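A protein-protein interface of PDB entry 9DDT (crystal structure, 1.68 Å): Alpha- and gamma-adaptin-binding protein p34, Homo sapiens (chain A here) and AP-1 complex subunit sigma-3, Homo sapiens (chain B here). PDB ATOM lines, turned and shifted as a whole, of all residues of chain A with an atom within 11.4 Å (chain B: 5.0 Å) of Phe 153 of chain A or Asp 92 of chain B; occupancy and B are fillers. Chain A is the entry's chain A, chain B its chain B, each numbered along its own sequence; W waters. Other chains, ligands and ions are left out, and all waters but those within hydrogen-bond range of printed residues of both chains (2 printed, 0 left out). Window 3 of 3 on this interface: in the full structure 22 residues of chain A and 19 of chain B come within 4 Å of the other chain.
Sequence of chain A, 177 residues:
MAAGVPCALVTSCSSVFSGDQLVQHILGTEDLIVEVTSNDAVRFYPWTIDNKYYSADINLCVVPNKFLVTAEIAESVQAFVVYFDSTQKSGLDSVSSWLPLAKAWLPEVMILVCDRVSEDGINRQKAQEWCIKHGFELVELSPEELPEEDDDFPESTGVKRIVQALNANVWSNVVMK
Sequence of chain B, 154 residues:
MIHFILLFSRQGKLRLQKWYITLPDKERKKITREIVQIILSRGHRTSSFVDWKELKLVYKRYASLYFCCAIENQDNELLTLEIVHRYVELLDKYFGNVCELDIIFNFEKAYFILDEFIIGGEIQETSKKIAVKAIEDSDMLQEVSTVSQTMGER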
ATOM      1  N   LYS A  52       1.882   9.165  36.726  1.00  0.00           N
ATOM      2  CA  LYS A  52       0.652   8.526  37.169  1.00  0.00           C
ATOM      3  C   LYS A  52       0.840   7.059  37.525  1.00  0.00           C
ATOM      4  O   LYS A  52       0.021   6.513  38.266  1.00  0.00           O
ATOM      5  CB  LYS A  52      -0.423   8.709  36.096  1.00  0.00           C
ATOM      6  CG  LYS A  52      -0.184   7.929  34.827  1.00  0.00           C
ATOM      7  CD  LYS A  52      -1.145   8.425  33.732  1.00  0.00           C
ATOM      8  CE  LYS A  52      -1.015   7.610  32.462  1.00  0.00           C
ATOM      9  NZ  LYS A  52      -2.164   7.692  31.504  1.00  0.00           N
ATOM     10  N   TYR A  53       1.916   6.422  37.063  1.00  0.00           N
ATOM     11  CA  TYR A  53       2.131   5.009  37.352  1.00  0.00           C
ATOM     12  C   TYR A  53       3.061   4.740  38.525  1.00  0.00           C
ATOM     13  O   TYR A  53       2.851   3.763  39.251  1.00  0.00           O
ATOM     14  CB  TYR A  53       2.681   4.307  36.111  1.00  0.00           C
ATOM     15  CG  TYR A  53       1.675   4.293  34.999  1.00  0.00           C
ATOM     16  CD1 TYR A  53       0.512   3.558  35.119  1.00  0.00           C
ATOM     17  CD2 TYR A  53       1.885   5.026  33.840  1.00  0.00           C
ATOM     18  CE1 TYR A  53      -0.427   3.529  34.100  1.00  0.00           C
ATOM     19  CE2 TYR A  53       0.966   5.005  32.814  1.00  0.00           C
ATOM     20  CZ  TYR A  53      -0.199   4.259  32.956  1.00  0.00           C
ATOM     21  OH  TYR A  53      -1.139   4.228  31.941  1.00  0.00           O
ATOM     22  N   PRO A 147       8.149  21.700  14.779  1.00  0.00           N
ATOM     23  CA  PRO A 147       7.487  20.573  14.117  1.00  0.00           C
ATOM     24  C   PRO A 147       6.394  21.042  13.167  1.00  0.00           C
ATOM     25  O   PRO A 147       5.864  22.149  13.278  1.00  0.00           O
ATOM     26  CB  PRO A 147       6.919  19.758  15.279  1.00  0.00           C
ATOM     27  CG  PRO A 147       6.702  20.757  16.359  1.00  0.00           C
ATOM     28  CD  PRO A 147       7.823  21.765  16.216  1.00  0.00           C
ATOM     29  N   GLU A 148       6.074  20.168  12.213  1.00  0.00           N
ATOM     30  CA  GLU A 148       5.127  20.491  11.152  1.00  0.00           C
ATOM     31  C   GLU A 148       3.749  20.742  11.757  1.00  0.00           C
ATOM     32  O   GLU A 148       3.326  20.045  12.682  1.00  0.00           O
ATOM     33  CB  GLU A 148       5.045  19.334  10.151  1.00  0.00           C
ATOM     34  CG  GLU A 148       6.367  18.920   9.475  1.00  0.00           C
ATOM     35  CD  GLU A 148       6.915  19.916   8.473  1.00  0.00           C
ATOM     36  OE1 GLU A 148       6.124  20.501   7.700  1.00  0.00           O
ATOM     37  OE2 GLU A 148       8.155  20.085   8.443  1.00  0.00           O
ATOM     38  N   GLU A 149       3.022  21.735  11.259  1.00  0.00           N
ATOM     39  CA  GLU A 149       1.708  22.101  11.847  1.00  0.00           C
ATOM     40  C   GLU A 149       0.658  20.997  11.646  1.00  0.00           C
ATOM     41  O   GLU A 149      -0.342  21.014  12.355  1.00  0.00           O
ATOM     42  CB  GLU A 149       1.294  23.458  11.273  1.00  0.00           C
ATOM     43  CG  GLU A 149       2.135  24.603  11.788  1.00  0.00           C
ATOM     44  CD  GLU A 149       3.383  24.889  10.974  1.00  0.00           C
ATOM     45  OE1 GLU A 149       4.096  25.847  11.320  1.00  0.00           O
ATOM     46  OE2 GLU A 149       3.638  24.155  10.003  1.00  0.00           O
ATOM     47  N   ASP A 150       0.895  20.076  10.712  1.00  0.00           N
ATOM     48  CA  ASP A 150      -0.061  18.962  10.463  1.00  0.00           C
ATOM     49  C   ASP A 150       0.513  17.651  11.010  1.00  0.00           C
ATOM     50  O   ASP A 150      -0.061  16.623  10.715  1.00  0.00           O
ATOM     51  CB  ASP A 150      -0.565  18.888   9.020  1.00  0.00           C
ATOM     52  CG  ASP A 150       0.524  18.906   7.969  1.00  0.00           C
ATOM     53  OD1 ASP A 150       1.705  18.914   8.350  1.00  0.00           O
ATOM     54  OD2 ASP A 150       0.167  18.912   6.779  1.00  0.00           O
ATOM     55  N   ASP A 151       1.579  17.725  11.796  1.00  0.00           N
ATOM     56  CA  ASP A 151       2.071  16.543  12.545  1.00  0.00           C
ATOM     57  C   ASP A 151       1.166  16.483  13.775  1.00  0.00           C
ATOM     58  O   ASP A 151       1.502  17.122  14.759  1.00  0.00           O
ATOM     59  CB  ASP A 151       3.548  16.715  12.872  1.00  0.00           C
ATOM     60  CG  ASP A 151       4.233  15.533  13.538  1.00  0.00           C
ATOM     61  OD1 ASP A 151       3.588  14.499  13.705  1.00  0.00           O
ATOM     62  OD2 ASP A 151       5.421  15.675  13.872  1.00  0.00           O
ATOM     63  N   ASP A 152       0.031  15.802  13.671  1.00  0.00           N
ATOM     64  CA  ASP A 152      -0.969  15.810  14.743  1.00  0.00           C
ATOM     65  C   ASP A 152      -0.548  15.042  15.989  1.00  0.00           C
ATOM     66  O   ASP A 152      -1.132  15.261  17.058  1.00  0.00           O
ATOM     67  CB  ASP A 152      -2.286  15.224  14.249  1.00  0.00           C
ATOM     68  CG  ASP A 152      -2.945  16.076  13.197  1.00  0.00           C
ATOM     69  OD1 ASP A 152      -2.692  17.305  13.162  1.00  0.00           O
ATOM     70  OD2 ASP A 152      -3.725  15.505  12.404  1.00  0.00           O
ATOM     71  N   PHE A 153       0.406  14.125  15.880  1.00  0.00           N
ATOM     72  CA  PHE A 153       0.937  13.398  17.033  1.00  0.00           C
ATOM     73  C   PHE A 153       2.445  13.583  17.033  1.00  0.00           C
ATOM     74  O   PHE A 153       3.205  12.652  16.752  1.00  0.00           O
ATOM     75  CB  PHE A 153       0.539  11.921  16.995  1.00  0.00           C
ATOM     76  CG  PHE A 153      -0.953  11.692  17.055  1.00  0.00           C
ATOM     77  CD1 PHE A 153      -1.731  11.791  15.909  1.00  0.00           C
ATOM     78  CD2 PHE A 153      -1.576  11.373  18.256  1.00  0.00           C
ATOM     79  CE1 PHE A 153      -3.105  11.584  15.956  1.00  0.00           C
ATOM     80  CE2 PHE A 153      -2.951  11.168  18.311  1.00  0.00           C
ATOM     81  CZ  PHE A 153      -3.712  11.270  17.157  1.00  0.00           C
ATOM     82  N   PRO A 154       2.911  14.790  17.336  1.00  0.00           N
ATOM     83  CA  PRO A 154       4.340  15.088  17.191  1.00  0.00           C
ATOM     84  C   PRO A 154       5.183  14.455  18.281  1.00  0.00           C
ATOM     85  O   PRO A 154       4.729  14.229  19.407  1.00  0.00           O
ATOM     86  CB  PRO A 154       4.391  16.618  17.285  1.00  0.00           C
ATOM     87  CG  PRO A 154       3.216  16.978  18.155  1.00  0.00           C
ATOM     88  CD  PRO A 154       2.151  15.927  17.891  1.00  0.00           C
ATOM     89  N   GLU A 155       6.446  14.251  17.934  1.00  0.00           N
ATOM     90  CA  GLU A 155       7.387  13.768  18.946  1.00  0.00           C
ATOM     91  C   GLU A 155       7.870  14.952  19.764  1.00  0.00           C
ATOM     92  O   GLU A 155       8.039  16.015  19.186  1.00  0.00           O
ATOM     93  CB  GLU A 155       8.648  13.211  18.290  1.00  0.00           C
ATOM     94  CG  GLU A 155       8.550  11.796  17.795  1.00  0.00           C
ATOM     95  CD  GLU A 155       9.859  11.322  17.194  1.00  0.00           C
ATOM     96  OE1 GLU A 155      10.492  10.457  17.790  1.00  0.00           O
ATOM     97  OE2 GLU A 155      10.241  11.836  16.141  1.00  0.00           O
ATOM     98  N   SER A 156       7.982  14.782  21.061  1.00  0.00           N
ATOM     99  CA  SER A 156       8.657  15.767  21.884  1.00  0.00           C
ATOM    100  C   SER A 156      10.123  15.834  21.484  1.00  0.00           C
ATOM    101  O   SER A 156      10.673  14.886  20.918  1.00  0.00           O
ATOM    102  CB  SER A 156       8.539  15.415  23.364  1.00  0.00           C
ATOM    103  OG  SER A 156       7.170  15.276  23.702  1.00  0.00           O
ATOM    104  N   THR A 157      10.748  16.968  21.800  1.00  0.00           N
ATOM    105  CA  THR A 157      12.147  17.209  21.481  1.00  0.00           C
ATOM    106  C   THR A 157      12.868  17.725  22.720  1.00  0.00           C
ATOM    107  O   THR A 157      12.257  18.074  23.736  1.00  0.00           O
ATOM    108  CB  THR A 157      12.303  18.228  20.335  1.00  0.00           C
ATOM    109  OG1 THR A 157      11.739  19.489  20.726  1.00  0.00           O
ATOM    110  CG2 THR A 157      11.616  17.733  19.068  1.00  0.00           C
ATOM    111  N   ARG A 161      11.846  15.737  25.811  1.00  0.00           N
ATOM    112  CA  ARG A 161      11.918  14.364  25.312  1.00  0.00           C
ATOM    113  C   ARG A 161      12.814  13.501  26.195  1.00  0.00           C
ATOM    114  O   ARG A 161      12.505  12.329  26.458  1.00  0.00           O
ATOM    115  CB  ARG A 161      12.402  14.365  23.857  1.00  0.00           C
ATOM    116  CG  ARG A 161      12.598  12.975  23.257  1.00  0.00           C
ATOM    117  CD  ARG A 161      11.325  12.126  23.321  1.00  0.00           C
ATOM    118  NE  ARG A 161      11.675  10.711  23.201  1.00  0.00           N
ATOM    119  CZ  ARG A 161      10.980   9.713  23.741  1.00  0.00           C
ATOM    120  NH1 ARG A 161       9.857   9.952  24.422  1.00  0.00           N
ATOM    121  NH2 ARG A 161      11.414   8.467  23.597  1.00  0.00           N
ATOM    122  N   GLN A 164      10.750  12.586  29.162  1.00  0.00           N
ATOM    123  CA  GLN A 164       9.775  11.570  28.774  1.00  0.00           C
ATOM    124  C   GLN A 164      10.428  10.192  28.679  1.00  0.00           C
ATOM    125  O   GLN A 164       9.893   9.198  29.188  1.00  0.00           O
ATOM    126  CB  GLN A 164       9.165  11.960  27.438  1.00  0.00           C
ATOM    127  CG  GLN A 164       8.038  11.109  26.972  1.00  0.00           C
ATOM    128  CD  GLN A 164       7.427  11.693  25.706  1.00  0.00           C
ATOM    129  OE1 GLN A 164       8.115  12.384  24.940  1.00  0.00           O
ATOM    130  NE2 GLN A 164       6.129  11.472  25.510  1.00  0.00           N
ATOM    131  N   ARG B  61       4.373   6.563  12.489  1.00  0.00           N
ATOM    132  CA  ARG B  61       4.818   7.055  13.784  1.00  0.00           C
ATOM    133  C   ARG B  61       3.753   7.949  14.398  1.00  0.00           C
ATOM    134  O   ARG B  61       3.241   8.863  13.740  1.00  0.00           O
ATOM    135  CB  ARG B  61       6.128   7.839  13.653  1.00  0.00           C
ATOM    136  CG  ARG B  61       6.724   8.285  14.980  1.00  0.00           C
ATOM    137  CD  ARG B  61       7.693   9.490  14.828  1.00  0.00           C
ATOM    138  NE  ARG B  61       7.140  10.548  13.984  1.00  0.00           N
ATOM    139  CZ  ARG B  61       6.215  11.420  14.383  1.00  0.00           C
ATOM    140  NH1 ARG B  61       5.735  11.368  15.622  1.00  0.00           N
ATOM    141  NH2 ARG B  61       5.762  12.336  13.538  1.00  0.00           N
ATOM    142  N   TYR B  62       3.409   7.667  15.651  1.00  0.00           N
ATOM    143  CA  TYR B  62       2.542   8.516  16.453  1.00  0.00           C
ATOM    144  C   TYR B  62       3.322   8.863  17.711  1.00  0.00           C
ATOM    145  O   TYR B  62       3.665   7.969  18.498  1.00  0.00           O
ATOM    146  CB  TYR B  62       1.215   7.825  16.795  1.00  0.00           C
ATOM    147  CG  TYR B  62       0.286   7.595  15.616  1.00  0.00           C
ATOM    148  CD1 TYR B  62       0.446   6.492  14.773  1.00  0.00           C
ATOM    149  CD2 TYR B  62      -0.756   8.475  15.348  1.00  0.00           C
ATOM    150  CE1 TYR B  62      -0.413   6.282  13.702  1.00  0.00           C
ATOM    151  CE2 TYR B  62      -1.613   8.277  14.282  1.00  0.00           C
ATOM    152  CZ  TYR B  62      -1.439   7.182  13.457  1.00  0.00           C
ATOM    153  OH  TYR B  62      -2.313   7.015  12.402  1.00  0.00           O
ATOM    154  N   ALA B  63       3.608  10.154  17.888  1.00  0.00           N
ATOM    155  CA  ALA B  63       4.485  10.644  18.960  1.00  0.00           C
ATOM    156  C   ALA B  63       5.796   9.862  18.850  1.00  0.00           C
ATOM    157  O   ALA B  63       6.379   9.799  17.760  1.00  0.00           O
ATOM    158  CB  ALA B  63       3.771  10.547  20.303  1.00  0.00           C
ATOM    159  N   HIS B  85      -4.806   3.966  12.486  1.00  0.00           N
ATOM    160  CA  HIS B  85      -5.205   5.259  13.029  1.00  0.00           C
ATOM    161  C   HIS B  85      -6.387   5.112  13.990  1.00  0.00           C
ATOM    162  O   HIS B  85      -6.443   5.783  15.030  1.00  0.00           O
ATOM    163  CB  HIS B  85      -5.545   6.211  11.882  1.00  0.00           C
ATOM    164  CG  HIS B  85      -5.786   7.608  12.339  1.00  0.00           C
ATOM    165  ND1 HIS B  85      -4.755   8.490  12.580  1.00  0.00           N
ATOM    166  CD2 HIS B  85      -6.926   8.260  12.654  1.00  0.00           C
ATOM    167  CE1 HIS B  85      -5.257   9.639  13.001  1.00  0.00           C
ATOM    168  NE2 HIS B  85      -6.571   9.525  13.056  1.00  0.00           N
ATOM    169  N   VAL B  88      -5.162   3.887  17.261  1.00  0.00           N
ATOM    170  CA  VAL B  88      -4.497   4.965  17.992  1.00  0.00           C
ATOM    171  C   VAL B  88      -5.538   5.874  18.623  1.00  0.00           C
ATOM    172  O   VAL B  88      -5.385   6.315  19.763  1.00  0.00           O
ATOM    173  CB  VAL B  88      -3.540   5.750  17.077  1.00  0.00           C
ATOM    174  CG1 VAL B  88      -3.058   7.019  17.781  1.00  0.00           C
ATOM    175  CG2 VAL B  88      -2.344   4.884  16.684  1.00  0.00           C
ATOM    176  N   GLU B  89      -6.616   6.165  17.896  1.00  0.00           N
ATOM    177  CA  GLU B  89      -7.680   6.994  18.473  1.00  0.00           C
ATOM    178  C   GLU B  89      -8.323   6.329  19.683  1.00  0.00           C
ATOM    179  O   GLU B  89      -8.681   7.006  20.656  1.00  0.00           O
ATOM    180  CB  GLU B  89      -8.736   7.302  17.424  1.00  0.00           C
ATOM    181  CG  GLU B  89      -8.280   8.264  16.351  1.00  0.00           C
ATOM    182  CD  GLU B  89      -9.410   8.612  15.404  1.00  0.00           C
ATOM    183  OE1 GLU B  89     -10.133   7.681  14.946  1.00  0.00           O
ATOM    184  OE2 GLU B  89      -9.594   9.824  15.147  1.00  0.00           O
ATOM    185  N   LEU B  90      -8.492   5.003  19.642  1.00  0.00           N
ATOM    186  CA  LEU B  90      -9.046   4.315  20.809  1.00  0.00           C
ATOM    187  C   LEU B  90      -8.106   4.430  22.010  1.00  0.00           C
ATOM    188  O   LEU B  90      -8.549   4.651  23.152  1.00  0.00           O
ATOM    189  CB  LEU B  90      -9.301   2.849  20.480  1.00  0.00           C
ATOM    190  CG  LEU B  90     -10.546   2.532  19.654  1.00  0.00           C
ATOM    191  CD1 LEU B  90     -10.506   1.081  19.181  1.00  0.00           C
ATOM    192  CD2 LEU B  90     -11.860   2.851  20.382  1.00  0.00           C
ATOM    193  N   LEU B  91      -6.800   4.274  21.766  1.00  0.00           N
ATOM    194  CA  LEU B  91      -5.817   4.460  22.837  1.00  0.00           C
ATOM    195  C   LEU B  91      -5.863   5.879  23.374  1.00  0.00           C
ATOM    196  O   LEU B  91      -5.819   6.096  24.589  1.00  0.00           O
ATOM    197  CB  LEU B  91      -4.407   4.137  22.341  1.00  0.00           C
ATOM    198  CG  LEU B  91      -4.176   2.694  21.917  1.00  0.00           C
ATOM    199  CD1 LEU B  91      -2.789   2.580  21.292  1.00  0.00           C
ATOM    200  CD2 LEU B  91      -4.312   1.754  23.114  1.00  0.00           C
ATOM    201  N   ASP B  92      -5.934   6.862  22.478  1.00  0.00           N
ATOM    202  CA  ASP B  92      -5.947   8.263  22.888  1.00  0.00           C
ATOM    203  C   ASP B  92      -7.188   8.563  23.718  1.00  0.00           C
ATOM    204  O   ASP B  92      -7.129   9.337  24.681  1.00  0.00           O
ATOM    205  CB  ASP B  92      -5.885   9.143  21.636  1.00  0.00           C
ATOM    206  CG  ASP B  92      -5.540  10.600  21.928  1.00  0.00           C
ATOM    207  OD1 ASP B  92      -5.114  10.919  23.058  1.00  0.00           O
ATOM    208  OD2 ASP B  92      -5.679  11.430  20.994  1.00  0.00           O
ATOM    209  N   LYS B  93      -8.324   7.951  23.362  1.00  0.00           N
ATOM    210  CA  LYS B  93      -9.550   8.129  24.140  1.00  0.00           C
ATOM    211  C   LYS B  93      -9.388   7.568  25.550  1.00  0.00           C
ATOM    212  O   LYS B  93      -9.766   8.217  26.534  1.00  0.00           O
ATOM    213  CB  LYS B  93     -10.739   7.462  23.438  1.00  0.00           C
ATOM    214  CG  LYS B  93     -12.101   7.822  24.054  1.00  0.00           C
ATOM    215  CD  LYS B  93     -13.276   7.100  23.379  1.00  0.00           C
ATOM    216  CE  LYS B  93     -14.497   6.957  24.319  1.00  0.00           C
ATOM    217  NZ  LYS B  93     -14.599   5.768  25.239  1.00  0.00           N
ATOM    218  N   TYR B  94      -8.826   6.358  25.678  1.00  0.00           N
ATOM    219  CA  TYR B  94      -8.722   5.786  27.022  1.00  0.00           C
ATOM    220  C   TYR B  94      -7.629   6.470  27.849  1.00  0.00           C
ATOM    221  O   TYR B  94      -7.849   6.846  29.007  1.00  0.00           O
ATOM    222  CB  TYR B  94      -8.451   4.284  26.973  1.00  0.00           C
ATOM    223  CG  TYR B  94      -8.262   3.749  28.366  1.00  0.00           C
ATOM    224  CD1 TYR B  94      -9.320   3.744  29.273  1.00  0.00           C
ATOM    225  CD2 TYR B  94      -7.018   3.335  28.817  1.00  0.00           C
ATOM    226  CE1 TYR B  94      -9.146   3.292  30.558  1.00  0.00           C
ATOM    227  CE2 TYR B  94      -6.839   2.884  30.111  1.00  0.00           C
ATOM    228  CZ  TYR B  94      -7.910   2.866  30.977  1.00  0.00           C
ATOM    229  OH  TYR B  94      -7.733   2.420  32.265  1.00  0.00           O
ATOM    230  N   PHE B  95      -6.429   6.598  27.299  1.00  0.00           N
ATOM    231  CA  PHE B  95      -5.300   7.081  28.080  1.00  0.00           C
ATOM    232  C   PHE B  95      -5.181   8.595  28.110  1.00  0.00           C
ATOM    233  O   PHE B  95      -4.349   9.116  28.863  1.00  0.00           O
ATOM    234  CB  PHE B  95      -3.992   6.494  27.543  1.00  0.00           C
ATOM    235  CG  PHE B  95      -3.862   5.016  27.753  1.00  0.00           C
ATOM    236  CD1 PHE B  95      -3.691   4.504  29.028  1.00  0.00           C
ATOM    237  CD2 PHE B  95      -3.867   4.136  26.678  1.00  0.00           C
ATOM    238  CE1 PHE B  95      -3.560   3.142  29.229  1.00  0.00           C
ATOM    239  CE2 PHE B  95      -3.739   2.776  26.876  1.00  0.00           C
ATOM    240  CZ  PHE B  95      -3.585   2.278  28.160  1.00  0.00           C
ATOM    241  N   GLY B  96      -5.956   9.310  27.296  1.00  0.00           N
ATOM    242  CA  GLY B  96      -5.857  10.753  27.220  1.00  0.00           C
ATOM    243  C   GLY B  96      -4.699  11.278  26.405  1.00  0.00           C
ATOM    244  O   GLY B  96      -4.585  12.501  26.237  1.00  0.00           O
ATOM    245  N   ASN B  97      -3.838  10.403  25.900  1.00  0.00           N
ATOM    246  CA  ASN B  97      -2.679  10.757  25.089  1.00  0.00           C
ATOM    247  C   ASN B  97      -2.181   9.458  24.465  1.00  0.00           C
ATOM    248  O   ASN B  97      -2.698   8.380  24.757  1.00  0.00           O
ATOM    249  CB  ASN B  97      -1.592  11.432  25.936  1.00  0.00           C
ATOM    250  CG  ASN B  97      -0.578  12.192  25.100  1.00  0.00           C
ATOM    251  OD1 ASN B  97      -0.681  12.256  23.875  1.00  0.00           O
ATOM    252  ND2 ASN B  97       0.412  12.777  25.766  1.00  0.00           N
ATOM    253  N   VAL B  98      -1.183   9.571  23.597  1.00  0.00           N
ATOM    254  CA  VAL B  98      -0.519   8.408  23.004  1.00  0.00           C
ATOM    255  C   VAL B  98       0.900   8.384  23.561  1.00  0.00           C
ATOM    256  O   VAL B  98       1.771   9.129  23.089  1.00  0.00           O
ATOM    257  CB  VAL B  98      -0.528   8.464  21.469  1.00  0.00           C
ATOM    258  CG1 VAL B  98       0.320   7.319  20.870  1.00  0.00           C
ATOM    259  CG2 VAL B  98      -1.960   8.446  20.937  1.00  0.00           C
HETATM  260  O   HOH W   1      -1.034   9.306  29.007  1.00  0.00           O
HETATM  261  O   HOH W   2       3.852  12.887  10.848  1.00  0.00           O
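Water W1 lies within hydrogen-bond range of NZ of Lys 52 of chain A (3.2 Å) and O of Phe 95 of chain B (3.3 Å). Water W2 lies within hydrogen-bond range of OD1 of Asp 151 of chain A (3.3 Å) and NH2 of Arg 61 of chain B (3.3 Å).
Hydrophobic or aromatic side chains of chain B that line the printed part of chain A: Tyr 62, Ala 63, Phe 95 and Val 98. Hydrophobic or aromatic side chains of chain A within 4 Å of the printed part of chain B: Tyr 53 and Phe 153. Among the printed residues, 11 pairs touch across the chains. Among the printed residues, Asp or Glu carboxylates within 4 Å of a Lys or Arg side-chain nitrogen of the other chain: Asp 151 of chain A with Arg 61 of chain B and Glu 155 of chain A with Arg 61 of chain B.
The backbone carbonyl oxygen (O) of Phe 153 of chain A lies within hydrogen-bond range of the backbone NH (N) of Ala 63 of chain B, 2.8 Å away. The side-chain carboxylate (OD1) of Asp 151 of chain A lies within salt-bridge range of the guanidinium group (NH2) of Arg 61 of chain B, 3.1 Å away. The backbone carbonyl oxygen (O) of Phe 153 of chain A lies within hydrogen-bond range of the guanidinium group (NH1) of Arg 61 of chain B, at 3.1 Å. The guanidinium group (NE) of Arg 61 of chain B is in salt-bridge range of the side-chain carboxylate (OE2) of Glu 155 of chain A, at 3.99 Å.
The backbone NH of Asn 97 of chain B is in hydrogen-bond range of the side-chain carboxylate of Asp 92 of chain B (3.2 Å). A ring nitrogen (ND1) of His 85 of chain B is in hydrogen-bond range of the side-chain hydroxyl (OH) of Tyr 62 of chain B. The backbone carbonyl oxygen (O) of Ala 63 of chain B lies within hydrogen-bond range of the guanidinium group (NH1) of Arg 61 of chain B (2.7 Å).
Phe 153 of chain A touches just these residues of chain B: Arg 61, Tyr 62, Ala 63, Asp 92 and Val 98. Of the printed residues of chain B, Glu 155 of chain A touches Arg 61 and Ala 63. Of the printed residues of chain A, Arg 61 of chain B touches Asp 151 (3.1 Å), Phe 153 (3.1 Å) and Glu 155 (3.6 Å). Of chain A, only Phe 153 (3.5 Å) comes within 4 Å of Tyr 62 of chain B. Of chain A, only Phe 153 (2.8 Å), Pro 154 (3.6 Å) and Glu 155 (2.9 Å) come within 4 Å of Ala 63 of chain B. Of the printed residues of chain A, Asp 92 of chain B touches Phe 153 (3.8 Å). Of the printed residues of chain A, Phe 95 of chain B touches Lys 52 and Tyr 53. No residue of chain A comes within 4 Å of Gly 96 of chain B. No residue of chain A comes within 4 Å of Asn 97 of chain B. Val 98 of chain B touches one residue of chain A. The nearest printed residue of chain A that does not touch Arg 61 of chain B is Pro 154 of chain A (4.1 Å).
Among the printed residues, pairs that only touch across the chains: Glu 155 of chain A with Ala 63 of chain B, Phe 153 of chain A with Tyr 62 of chain B, Pro 154 of chain A with Ala 63 of chain B, Lys 52 of chain A with Phe 95 of chain B, Tyr 53 of chain A with Phe 95 of chain B, Phe 153 of chain A with Asp 92 of chain B and Phe 153 of chain A with Val 98 of chain B.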
